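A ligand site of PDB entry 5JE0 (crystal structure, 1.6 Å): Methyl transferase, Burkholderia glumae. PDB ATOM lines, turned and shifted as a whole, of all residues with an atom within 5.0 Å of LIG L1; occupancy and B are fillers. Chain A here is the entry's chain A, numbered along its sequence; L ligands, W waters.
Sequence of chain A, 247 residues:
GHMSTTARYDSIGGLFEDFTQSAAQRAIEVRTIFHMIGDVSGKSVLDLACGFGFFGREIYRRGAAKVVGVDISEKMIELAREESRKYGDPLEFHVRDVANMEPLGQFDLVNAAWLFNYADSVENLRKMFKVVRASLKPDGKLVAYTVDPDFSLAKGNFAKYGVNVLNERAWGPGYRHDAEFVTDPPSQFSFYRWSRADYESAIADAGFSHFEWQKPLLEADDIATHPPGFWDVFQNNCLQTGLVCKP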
ATOM      1  N   TYR A   9       2.120 -18.959  -2.226  1.00  0.00           N
ATOM      2  CA  TYR A   9       2.817 -18.507  -3.413  1.00  0.00           C
ATOM      3  C   TYR A   9       2.064 -17.427  -4.164  1.00  0.00           C
ATOM      4  O   TYR A   9       2.610 -16.869  -5.128  1.00  0.00           O
ATOM      5  CB  TYR A   9       3.126 -19.699  -4.340  1.00  0.00           C
ATOM      6  CG  TYR A   9       4.401 -20.416  -3.956  1.00  0.00           C
ATOM      7  CD1 TYR A   9       5.552 -20.321  -4.745  1.00  0.00           C
ATOM      8  CD2 TYR A   9       4.467 -21.168  -2.791  1.00  0.00           C
ATOM      9  CE1 TYR A   9       6.736 -20.990  -4.378  1.00  0.00           C
ATOM     10  CE2 TYR A   9       5.632 -21.833  -2.411  1.00  0.00           C
ATOM     11  CZ  TYR A   9       6.757 -21.737  -3.209  1.00  0.00           C
ATOM     12  OH  TYR A   9       7.916 -22.390  -2.835  1.00  0.00           O
ATOM     13  N   PHE A  16       9.379 -16.432  -8.047  1.00  0.00           N
ATOM     14  CA  PHE A  16       9.878 -17.801  -7.972  1.00  0.00           C
ATOM     15  C   PHE A  16      10.716 -18.142  -9.198  1.00  0.00           C
ATOM     16  O   PHE A  16      11.755 -18.802  -9.078  1.00  0.00           O
ATOM     17  CB  PHE A  16       8.727 -18.800  -7.791  1.00  0.00           C
ATOM     18  CG  PHE A  16       9.170 -20.226  -7.843  1.00  0.00           C
ATOM     19  CD1 PHE A  16       9.846 -20.795  -6.756  1.00  0.00           C
ATOM     20  CD2 PHE A  16       8.963 -20.999  -8.973  1.00  0.00           C
ATOM     21  CE1 PHE A  16      10.280 -22.106  -6.805  1.00  0.00           C
ATOM     22  CE2 PHE A  16       9.397 -22.310  -9.022  1.00  0.00           C
ATOM     23  CZ  PHE A  16      10.058 -22.869  -7.935  1.00  0.00           C
ATOM     24  N   THR A  20      14.601 -19.433  -9.593  1.00  0.00           N
ATOM     25  CA  THR A  20      15.090 -20.585 -10.337  1.00  0.00           C
ATOM     26  C   THR A  20      16.176 -20.192 -11.323  1.00  0.00           C
ATOM     27  O   THR A  20      16.985 -21.043 -11.698  1.00  0.00           O
ATOM     28  CB  THR A  20      13.949 -21.310 -11.067  1.00  0.00           C
ATOM     29  OG1 THR A  20      13.459 -20.516 -12.157  1.00  0.00           O
ATOM     30  CG2 THR A  20      12.805 -21.665 -10.084  1.00  0.00           C
ATOM     31  N   ARG A  26      19.608 -24.961  -8.449  1.00  0.00           N
ATOM     32  CA  ARG A  26      18.565 -25.318  -9.399  1.00  0.00           C
ATOM     33  C   ARG A  26      19.112 -26.141 -10.566  1.00  0.00           C
ATOM     34  O   ARG A  26      18.464 -27.078 -11.020  1.00  0.00           O
ATOM     35  CB  ARG A  26      17.869 -24.063  -9.906  1.00  0.00           C
ATOM     36  CG  ARG A  26      16.687 -24.348 -10.862  1.00  0.00           C
ATOM     37  CD  ARG A  26      15.539 -25.101 -10.173  1.00  0.00           C
ATOM     38  NE  ARG A  26      14.357 -25.067 -11.035  1.00  0.00           N
ATOM     39  CZ  ARG A  26      13.121 -25.400 -10.683  1.00  0.00           C
ATOM     40  NH1 ARG A  26      12.839 -25.821  -9.449  1.00  0.00           N
ATOM     41  NH2 ARG A  26      12.148 -25.300 -11.573  1.00  0.00           N
ATOM     42  N   GLU A  29      19.410 -29.740  -9.311  1.00  0.00           N
ATOM     43  CA  GLU A  29      18.149 -30.449  -9.138  1.00  0.00           C
ATOM     44  C   GLU A  29      17.481 -30.730 -10.479  1.00  0.00           C
ATOM     45  O   GLU A  29      16.913 -31.818 -10.666  1.00  0.00           O
ATOM     46  CB  GLU A  29      17.226 -29.669  -8.185  1.00  0.00           C
ATOM     47  CG  GLU A  29      16.385 -28.569  -8.751  1.00  0.00           C
ATOM     48  CD  GLU A  29      15.700 -27.756  -7.662  1.00  0.00           C
ATOM     49  OE1 GLU A  29      16.358 -27.458  -6.643  1.00  0.00           O
ATOM     50  OE2 GLU A  29      14.505 -27.419  -7.824  1.00  0.00           O
ATOM     51  N   LEU A  48       2.837 -32.329 -10.394  1.00  0.00           N
ATOM     52  CA  LEU A  48       2.182 -31.896  -9.161  1.00  0.00           C
ATOM     53  C   LEU A  48       3.025 -30.853  -8.431  1.00  0.00           C
ATOM     54  O   LEU A  48       4.257 -30.921  -8.413  1.00  0.00           O
ATOM     55  CB  LEU A  48       1.938 -33.080  -8.232  1.00  0.00           C
ATOM     56  CG  LEU A  48       1.059 -34.196  -8.797  1.00  0.00           C
ATOM     57  CD1 LEU A  48       0.948 -35.324  -7.772  1.00  0.00           C
ATOM     58  CD2 LEU A  48      -0.338 -33.674  -9.123  1.00  0.00           C
ATOM     59  N   ALA A  49       2.336 -29.916  -7.778  1.00  0.00           N
ATOM     60  CA  ALA A  49       2.970 -28.702  -7.235  1.00  0.00           C
ATOM     61  C   ALA A  49       3.762 -28.019  -8.349  1.00  0.00           C
ATOM     62  O   ALA A  49       4.941 -27.663  -8.188  1.00  0.00           O
ATOM     63  CB  ALA A  49       3.867 -29.009  -6.031  1.00  0.00           C
ATOM     64  N   CYS A  50       3.090 -27.836  -9.493  1.00  0.00           N
ATOM     65  CA  CYS A  50       3.797 -27.546 -10.732  1.00  0.00           C
ATOM     66  C   CYS A  50       4.351 -26.130 -10.808  1.00  0.00           C
ATOM     67  O   CYS A  50       5.164 -25.866 -11.701  1.00  0.00           O
ATOM     68  CB  CYS A  50       2.875 -27.812 -11.925  1.00  0.00           C
ATOM     69  SG  CYS A  50       1.406 -26.738 -12.024  1.00  0.00           S
ATOM     70  N   GLY A  51       3.911 -25.213  -9.959  1.00  0.00           N
ATOM     71  CA  GLY A  51       4.426 -23.849 -10.051  1.00  0.00           C
ATOM     72  C   GLY A  51       3.932 -23.175 -11.317  1.00  0.00           C
ATOM     73  O   GLY A  51       2.763 -23.300 -11.701  1.00  0.00           O
ATOM     74  N   PHE A  52       4.822 -22.448 -11.987  1.00  0.00           N
ATOM     75  CA  PHE A  52       4.473 -21.903 -13.290  1.00  0.00           C
ATOM     76  C   PHE A  52       4.568 -22.952 -14.387  1.00  0.00           C
ATOM     77  O   PHE A  52       4.390 -22.635 -15.568  1.00  0.00           O
ATOM     78  CB  PHE A  52       5.346 -20.678 -13.627  1.00  0.00           C
ATOM     79  CG  PHE A  52       6.826 -20.943 -13.664  1.00  0.00           C
ATOM     80  CD1 PHE A  52       7.433 -21.433 -14.815  1.00  0.00           C
ATOM     81  CD2 PHE A  52       7.620 -20.659 -12.560  1.00  0.00           C
ATOM     82  CE1 PHE A  52       8.791 -21.653 -14.866  1.00  0.00           C
ATOM     83  CE2 PHE A  52       8.992 -20.880 -12.606  1.00  0.00           C
ATOM     84  CZ  PHE A  52       9.578 -21.382 -13.761  1.00  0.00           C
ATOM     85  N   PHE A  54       7.254 -25.369 -14.801  1.00  0.00           N
ATOM     86  CA  PHE A  54       8.581 -25.583 -15.389  1.00  0.00           C
ATOM     87  C   PHE A  54       8.791 -27.022 -15.835  1.00  0.00           C
ATOM     88  O   PHE A  54       9.195 -27.271 -16.979  1.00  0.00           O
ATOM     89  CB  PHE A  54       9.696 -25.197 -14.436  1.00  0.00           C
ATOM     90  CG  PHE A  54      11.059 -25.574 -14.974  1.00  0.00           C
ATOM     91  CD1 PHE A  54      11.608 -24.847 -16.020  1.00  0.00           C
ATOM     92  CD2 PHE A  54      11.752 -26.678 -14.504  1.00  0.00           C
ATOM     93  CE1 PHE A  54      12.841 -25.192 -16.570  1.00  0.00           C
ATOM     94  CE2 PHE A  54      13.003 -27.017 -15.062  1.00  0.00           C
ATOM     95  CZ  PHE A  54      13.531 -26.268 -16.090  1.00  0.00           C
ATOM     96  N   PHE A  55       8.584 -27.979 -14.931  1.00  0.00           N
ATOM     97  CA  PHE A  55       8.945 -29.354 -15.242  1.00  0.00           C
ATOM     98  C   PHE A  55       8.012 -29.956 -16.278  1.00  0.00           C
ATOM     99  O   PHE A  55       8.461 -30.559 -17.254  1.00  0.00           O
ATOM    100  CB  PHE A  55       9.019 -30.214 -13.983  1.00  0.00           C
ATOM    101  CG  PHE A  55      10.249 -29.956 -13.204  1.00  0.00           C
ATOM    102  CD1 PHE A  55      11.477 -30.418 -13.667  1.00  0.00           C
ATOM    103  CD2 PHE A  55      10.214 -29.154 -12.083  1.00  0.00           C
ATOM    104  CE1 PHE A  55      12.649 -30.129 -12.964  1.00  0.00           C
ATOM    105  CE2 PHE A  55      11.381 -28.862 -11.389  1.00  0.00           C
ATOM    106  CZ  PHE A  55      12.599 -29.351 -11.842  1.00  0.00           C
ATOM    107  N   VAL A  70      -0.801 -29.397 -11.697  1.00  0.00           N
ATOM    108  CA  VAL A  70      -1.659 -29.074 -10.548  1.00  0.00           C
ATOM    109  C   VAL A  70      -0.845 -28.255  -9.559  1.00  0.00           C
ATOM    110  O   VAL A  70       0.269 -28.637  -9.210  1.00  0.00           O
ATOM    111  CB  VAL A  70      -2.213 -30.336  -9.857  1.00  0.00           C
ATOM    112  CG1 VAL A  70      -3.176 -29.964  -8.729  1.00  0.00           C
ATOM    113  CG2 VAL A  70      -2.881 -31.292 -10.863  1.00  0.00           C
ATOM    114  N   ASP A  71      -1.427 -27.156  -9.085  1.00  0.00           N
ATOM    115  CA  ASP A  71      -0.818 -26.353  -8.032  1.00  0.00           C
ATOM    116  C   ASP A  71      -1.938 -25.748  -7.186  1.00  0.00           C
ATOM    117  O   ASP A  71      -3.034 -25.482  -7.685  1.00  0.00           O
ATOM    118  CB  ASP A  71       0.077 -25.245  -8.629  1.00  0.00           C
ATOM    119  CG  ASP A  71       1.107 -24.733  -7.638  1.00  0.00           C
ATOM    120  OD1 ASP A  71       2.275 -25.185  -7.673  1.00  0.00           O
ATOM    121  OD2 ASP A  71       0.732 -23.908  -6.781  1.00  0.00           O
ATOM    122  N   ILE A  72      -1.657 -25.543  -5.909  1.00  0.00           N
ATOM    123  CA  ILE A  72      -2.628 -24.979  -4.993  1.00  0.00           C
ATOM    124  C   ILE A  72      -2.766 -23.461  -5.157  1.00  0.00           C
ATOM    125  O   ILE A  72      -3.752 -22.877  -4.689  1.00  0.00           O
ATOM    126  CB  ILE A  72      -2.225 -25.372  -3.557  1.00  0.00           C
ATOM    127  CG1 ILE A  72      -3.400 -25.188  -2.601  1.00  0.00           C
ATOM    128  CG2 ILE A  72      -1.039 -24.536  -3.094  1.00  0.00           C
ATOM    129  CD1 ILE A  72      -3.058 -25.525  -1.162  1.00  0.00           C
ATOM    130  N   SER A  73      -1.812 -22.816  -5.816  1.00  0.00           N
ATOM    131  CA  SER A  73      -1.786 -21.357  -5.913  1.00  0.00           C
ATOM    132  C   SER A  73      -2.431 -20.891  -7.213  1.00  0.00           C
ATOM    133  O   SER A  73      -1.963 -21.227  -8.300  1.00  0.00           O
ATOM    134  CB  SER A  73      -0.351 -20.842  -5.815  1.00  0.00           C
ATOM    135  OG  SER A  73      -0.281 -19.483  -6.215  1.00  0.00           O
ATOM    136  N   MET A  76       0.237 -18.934  -9.193  1.00  0.00           N
ATOM    137  CA  MET A  76       1.206 -19.713  -9.958  1.00  0.00           C
ATOM    138  C   MET A  76       0.542 -20.349 -11.168  1.00  0.00           C
ATOM    139  O   MET A  76       1.142 -20.425 -12.253  1.00  0.00           O
ATOM    140  CB  MET A  76       1.870 -20.768  -9.066  1.00  0.00           C
ATOM    141  CG  MET A  76       2.574 -20.176  -7.868  1.00  0.00           C
ATOM    142  SD  MET A  76       3.783 -18.894  -8.282  1.00  0.00           S
ATOM    143  CE  MET A  76       5.044 -19.835  -9.130  1.00  0.00           C
ATOM    144  N   ARG A  96      -5.558 -26.991  -7.328  1.00  0.00           N
ATOM    145  CA  ARG A  96      -6.014 -27.940  -6.317  1.00  0.00           C
ATOM    146  C   ARG A  96      -4.917 -28.133  -5.274  1.00  0.00           C
ATOM    147  O   ARG A  96      -3.726 -28.080  -5.577  1.00  0.00           O
ATOM    148  CB  ARG A  96      -6.378 -29.306  -6.914  1.00  0.00           C
ATOM    149  CG  ARG A  96      -7.470 -29.235  -7.971  1.00  0.00           C
ATOM    150  CD  ARG A  96      -7.759 -30.547  -8.666  1.00  0.00           C
ATOM    151  NE  ARG A  96      -8.808 -30.304  -9.651  1.00  0.00           N
ATOM    152  CZ  ARG A  96      -9.330 -31.230 -10.456  1.00  0.00           C
ATOM    153  NH1 ARG A  96      -8.881 -32.484 -10.391  1.00  0.00           N
ATOM    154  NH2 ARG A  96     -10.281 -30.899 -11.327  1.00  0.00           N
ATOM    155  N   ASP A  97      -5.351 -28.339  -4.034  1.00  0.00           N
ATOM    156  CA  ASP A  97      -4.487 -28.933  -3.025  1.00  0.00           C
ATOM    157  C   ASP A  97      -4.347 -30.426  -3.316  1.00  0.00           C
ATOM    158  O   ASP A  97      -5.329 -31.173  -3.277  1.00  0.00           O
ATOM    159  CB  ASP A  97      -5.107 -28.688  -1.642  1.00  0.00           C
ATOM    160  CG  ASP A  97      -4.266 -29.249  -0.492  1.00  0.00           C
ATOM    161  OD1 ASP A  97      -3.340 -30.062  -0.697  1.00  0.00           O
ATOM    162  OD2 ASP A  97      -4.578 -28.865   0.663  1.00  0.00           O
ATOM    163  N   VAL A  98      -3.131 -30.862  -3.646  1.00  0.00           N
ATOM    164  CA  VAL A  98      -2.946 -32.234  -4.082  1.00  0.00           C
ATOM    165  C   VAL A  98      -3.372 -33.240  -3.021  1.00  0.00           C
ATOM    166  O   VAL A  98      -3.809 -34.339  -3.345  1.00  0.00           O
ATOM    167  CB  VAL A  98      -1.479 -32.418  -4.527  1.00  0.00           C
ATOM    168  CG1 VAL A  98      -1.139 -33.890  -4.724  1.00  0.00           C
ATOM    169  CG2 VAL A  98      -1.321 -31.662  -5.842  1.00  0.00           C
ATOM    170  N   ALA A  99      -3.259 -32.876  -1.734  1.00  0.00           N
ATOM    171  CA  ALA A  99      -3.643 -33.818  -0.690  1.00  0.00           C
ATOM    172  C   ALA A  99      -5.113 -34.192  -0.774  1.00  0.00           C
ATOM    173  O   ALA A  99      -5.501 -35.285  -0.353  1.00  0.00           O
ATOM    174  CB  ALA A  99      -3.352 -33.233   0.693  1.00  0.00           C
ATOM    175  N   ALA A 113       8.022 -32.201  -8.072  1.00  0.00           N
ATOM    176  CA  ALA A 113       9.186 -31.443  -7.607  1.00  0.00           C
ATOM    177  C   ALA A 113       8.707 -30.421  -6.586  1.00  0.00           C
ATOM    178  O   ALA A 113       8.037 -29.442  -6.940  1.00  0.00           O
ATOM    179  CB  ALA A 113       9.918 -30.783  -8.765  1.00  0.00           C
ATOM    180  N   TRP A 114       9.043 -30.657  -5.315  1.00  0.00           N
ATOM    181  CA  TRP A 114       8.696 -29.772  -4.196  1.00  0.00           C
ATOM    182  C   TRP A 114       7.196 -29.805  -3.903  1.00  0.00           C
ATOM    183  O   TRP A 114       6.568 -28.762  -3.704  1.00  0.00           O
ATOM    184  CB  TRP A 114       9.192 -28.356  -4.441  1.00  0.00           C
ATOM    185  CG  TRP A 114      10.661 -28.329  -4.731  1.00  0.00           C
ATOM    186  CD1 TRP A 114      11.249 -27.982  -5.898  1.00  0.00           C
ATOM    187  CD2 TRP A 114      11.701 -28.700  -3.839  1.00  0.00           C
ATOM    188  NE1 TRP A 114      12.617 -28.097  -5.793  1.00  0.00           N
ATOM    189  CE2 TRP A 114      12.926 -28.535  -4.531  1.00  0.00           C
ATOM    190  CE3 TRP A 114      11.720 -29.156  -2.501  1.00  0.00           C
ATOM    191  CZ2 TRP A 114      14.169 -28.788  -3.933  1.00  0.00           C
ATOM    192  CZ3 TRP A 114      12.937 -29.418  -1.915  1.00  0.00           C
ATOM    193  CH2 TRP A 114      14.147 -29.236  -2.629  1.00  0.00           C
ATOM    194  N   LEU A 115       6.637 -31.010  -3.880  1.00  0.00           N
ATOM    195  CA  LEU A 115       5.283 -31.266  -3.391  1.00  0.00           C
ATOM    196  C   LEU A 115       5.273 -31.669  -1.914  1.00  0.00           C
ATOM    197  O   LEU A 115       4.563 -31.060  -1.097  1.00  0.00           O
ATOM    198  CB  LEU A 115       4.613 -32.360  -4.222  1.00  0.00           C
ATOM    199  CG  LEU A 115       3.289 -32.872  -3.635  1.00  0.00           C
ATOM    200  CD1 LEU A 115       2.219 -31.786  -3.612  1.00  0.00           C
ATOM    201  CD2 LEU A 115       2.788 -34.072  -4.415  1.00  0.00           C
ATOM    202  N   TYR A 118       5.377 -29.713   1.399  1.00  0.00           N
ATOM    203  CA  TYR A 118       4.291 -28.843   1.782  1.00  0.00           C
ATOM    204  C   TYR A 118       3.190 -29.581   2.533  1.00  0.00           C
ATOM    205  O   TYR A 118       2.237 -28.935   2.988  1.00  0.00           O
ATOM    206  CB  TYR A 118       3.729 -28.132   0.542  1.00  0.00           C
ATOM    207  CG  TYR A 118       4.722 -27.129   0.060  1.00  0.00           C
ATOM    208  CD1 TYR A 118       4.817 -25.883   0.668  1.00  0.00           C
ATOM    209  CD2 TYR A 118       5.633 -27.442  -0.950  1.00  0.00           C
ATOM    210  CE1 TYR A 118       5.784 -24.967   0.271  1.00  0.00           C
ATOM    211  CE2 TYR A 118       6.597 -26.540  -1.338  1.00  0.00           C
ATOM    212  CZ  TYR A 118       6.681 -25.311  -0.716  1.00  0.00           C
ATOM    213  OH  TYR A 118       7.652 -24.397  -1.105  1.00  0.00           O
ATOM    214  N   MET A 128      -1.085 -37.537   0.282  1.00  0.00           N
ATOM    215  CA  MET A 128      -0.483 -37.190  -1.000  1.00  0.00           C
ATOM    216  C   MET A 128       0.069 -38.421  -1.709  1.00  0.00           C
ATOM    217  O   MET A 128      -0.131 -38.589  -2.914  1.00  0.00           O
ATOM    218  CB  MET A 128       0.628 -36.163  -0.794  1.00  0.00           C
ATOM    219  CG  MET A 128       0.104 -34.777  -0.387  1.00  0.00           C
ATOM    220  SD  MET A 128       1.536 -33.689  -0.309  1.00  0.00           S
ATOM    221  CE  MET A 128       0.838 -32.079   0.012  1.00  0.00           C
HETATM  222  N1  LIG L   1       7.329 -27.627  -9.161  1.00  0.00           N
HETATM  223  C1  LIG L   1       7.673 -26.191  -9.421  1.00  0.00           C
HETATM  224  C2  LIG L   1       7.366 -25.261  -8.240  1.00  0.00           C
HETATM  225  C3  LIG L   1       7.970 -25.714  -6.900  1.00  0.00           C
HETATM  226  S1  LIG L   1       7.692 -24.526  -5.624  1.00  0.00           S
HETATM  227  C4  LIG L   1       9.117 -26.061  -9.797  1.00  0.00           C
HETATM  228  O1  LIG L   1       9.479 -25.235 -10.672  1.00  0.00           O
HETATM  229  O2  LIG L   1       9.942 -26.788  -9.232  1.00  0.00           O
HETATM  230  C5  LIG L   1       6.449 -25.360  -4.679  1.00  0.00           C
HETATM  231  C6  LIG L   1       5.061 -25.252  -5.308  1.00  0.00           C
HETATM  232  O3  LIG L   1       4.191 -26.159  -4.608  1.00  0.00           O
HETATM  233  C7  LIG L   1       4.432 -23.856  -5.231  1.00  0.00           C
HETATM  234  O4  LIG L   1       4.019 -23.415  -6.564  1.00  0.00           O
HETATM  235  C8  LIG L   1       3.222 -24.074  -4.326  1.00  0.00           C
HETATM  236  O5  LIG L   1       2.096 -23.232  -4.592  1.00  0.00           O
HETATM  237  C9  LIG L   1       2.913 -25.536  -4.580  1.00  0.00           C
HETATM  238  N2  LIG L   1       2.173 -26.203  -3.491  1.00  0.00           N
HETATM  239  C10 LIG L   1       2.377 -26.071  -2.156  1.00  0.00           C
HETATM  240  N3  LIG L   1       1.506 -26.852  -1.478  1.00  0.00           N
HETATM  241  C11 LIG L   1       0.754 -27.500  -2.356  1.00  0.00           C
HETATM  242  C12 LIG L   1      -0.336 -28.479  -2.300  1.00  0.00           C
HETATM  243  N4  LIG L   1      -0.809 -28.923  -1.095  1.00  0.00           N
HETATM  244  N5  LIG L   1      -0.870 -28.910  -3.476  1.00  0.00           N
HETATM  245  C13 LIG L   1      -0.406 -28.469  -4.676  1.00  0.00           C
HETATM  246  N6  LIG L   1       0.572 -27.574  -4.801  1.00  0.00           N
HETATM  247  C14 LIG L   1       1.194 -27.078  -3.691  1.00  0.00           C
HETATM  248  C1  LG2 L   2      13.238 -25.666  -2.597  1.00  0.00           C
HETATM  249  N1  LG2 L   2      14.438 -25.819  -2.053  1.00  0.00           N
HETATM  250  N2  LG2 L   2      14.513 -26.132  -0.799  1.00  0.00           N
HETATM  251  C2  LG2 L   2      13.446 -26.301  -0.044  1.00  0.00           C
HETATM  252  N3  LG2 L   2      12.220 -26.159  -0.506  1.00  0.00           N
HETATM  253  C3  LG2 L   2      12.090 -25.839  -1.797  1.00  0.00           C
HETATM  254  C4  LG2 L   2      10.777 -25.645  -2.432  1.00  0.00           C
HETATM  255  O1  LG2 L   2       9.728 -25.802  -1.825  1.00  0.00           O
HETATM  256  N4  LG2 L   2      10.733 -25.315  -3.757  1.00  0.00           N
HETATM  257  C5  LG2 L   2      11.870 -25.171  -4.477  1.00  0.00           C
HETATM  258  O2  LG2 L   2      11.810 -24.872  -5.660  1.00  0.00           O
HETATM  259  N5  LG2 L   2      13.089 -25.329  -3.944  1.00  0.00           N
HETATM  260  O   HOH W   1       6.978 -27.823 -12.364  1.00  0.00           O
HETATM  261  O   HOH W   2       1.158 -21.796  -2.371  1.00  0.00           O
HETATM  262  O   HOH W   3       7.623 -23.990 -12.210  1.00  0.00           O
HETATM  263  O   HOH W   4      -0.269 -28.569   1.668  1.00  0.00           O
HETATM  264  O   HOH W   5       6.491 -30.327  -9.799  1.00  0.00           O
HETATM  265  O   HOH W   6       6.189 -22.261  -7.655  1.00  0.00           O
HETATM  266  O   HOH W   7       0.852 -25.459   0.925  1.00  0.00           O
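The backbone carbonyl oxygen (O) of Ala 49 sits at hydrogen-bond distance from a nitrogen (N1) of LIG L1, at 2.6 Å. An oxygen (O5) of LIG L1 sits at hydrogen-bond distance from the side-chain carboxylate (OD2) of Asp 71 (2.7 Å). OD1 of Asp 97 lies within hydrogen-bond range of N4 of LIG L1, at 2.8 Å. An oxygen (O1) of LIG L1 is in salt-bridge range of the guanidinium group (NH2) of Arg 26. N1 of LIG L1 lies within hydrogen-bond range of O of Ala 113 (3.0 Å). N of Val 98 lies within hydrogen-bond range of N5 of LIG L1, 3.0 Å away. A nitrogen (N6) of LIG L1 sits at hydrogen-bond distance from the backbone NH (N) of Ile 72 (3.2 Å). OH of Tyr 9 lies close to S1 of LIG L1 (3.5 Å). The side-chain hydroxyl (OH) of Tyr 118 is in hydrogen-bond range of an oxygen (O1) of LG2 L2. An oxygen (O2) of LG2 L2 sits close to the indole nitrogen (NE1) of Trp 114.
Water W3 lies within hydrogen-bond range of O1 of LIG L1 (2.7 Å), N of Phe 54 (3.0 Å), O of Cys 50 (3.1 Å) and N of Phe 52 (3.2 Å). Water W2 bridges O5 of LIG L1 and N of Tyr 9. Water W4 bridges a nitrogen (N4) of LIG L1 and the backbone carbonyl oxygen of Tyr 118. Water W5 lies within hydrogen-bond range of O of Leu 48, N1 of LIG L1, N of Ala 113 and O of Ala 49. Water W1 lies within hydrogen-bond range of the backbone carbonyl oxygen (O) of Cys 50, the backbone NH (N) of Phe 55, a nitrogen (N1) of LIG L1 and the backbone NH (N) of Phe 54.
Merely in contact with LIG L1: Phe 16 (3.4 Å), Cys 50 (3.4 Å), Gly 51 (3.5 Å), Phe 54 (3.8 Å), Phe 55 (3.3 Å), Ser 73 (3.6 Å), Met 76 (3.8 Å), Arg 96 (3.5 Å), Trp 114 (3.5 Å), Tyr 118 (3.3 Å) and Met 128 (3.7 Å). Hydrophobic or aromatic side chains that line LIG L1: Tyr 9, Phe 16, Ala 49, Phe 54, Phe 55, Ile 72, Met 76, Val 98, Trp 114, Tyr 118 and Met 128.
A sulfur (S1) of LIG L1 lies close to a nitrogen (N4) of LG2 L2 (3.7 Å).
N of Ala 49 sits at hydrogen-bond distance from O of Val 70 (2.8 Å). N of Cys 50 lies within hydrogen-bond range of OD1 of Asp 71. N of Arg 96 is in hydrogen-bond range of O of Asp 71, at 3.0 Å. OD1 of Asp 71 sits at hydrogen-bond distance from N of Gly 51 (2.8 Å). The side-chain carboxylate of Asp 97 lies within hydrogen-bond range of the backbone NH of Ala 99 (3.0 Å). The guanidinium group of Arg 26 is in salt-bridge range of the side-chain carboxylate of Glu 29 (2.8 Å). The backbone NH (N) of Ile 72 is in hydrogen-bond range of the backbone carbonyl oxygen (O) of Arg 96 (3.3 Å). The side-chain hydroxyl of Tyr 9 sits at hydrogen-bond distance from the side-chain hydroxyl of Tyr 118, 2.7 Å away.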
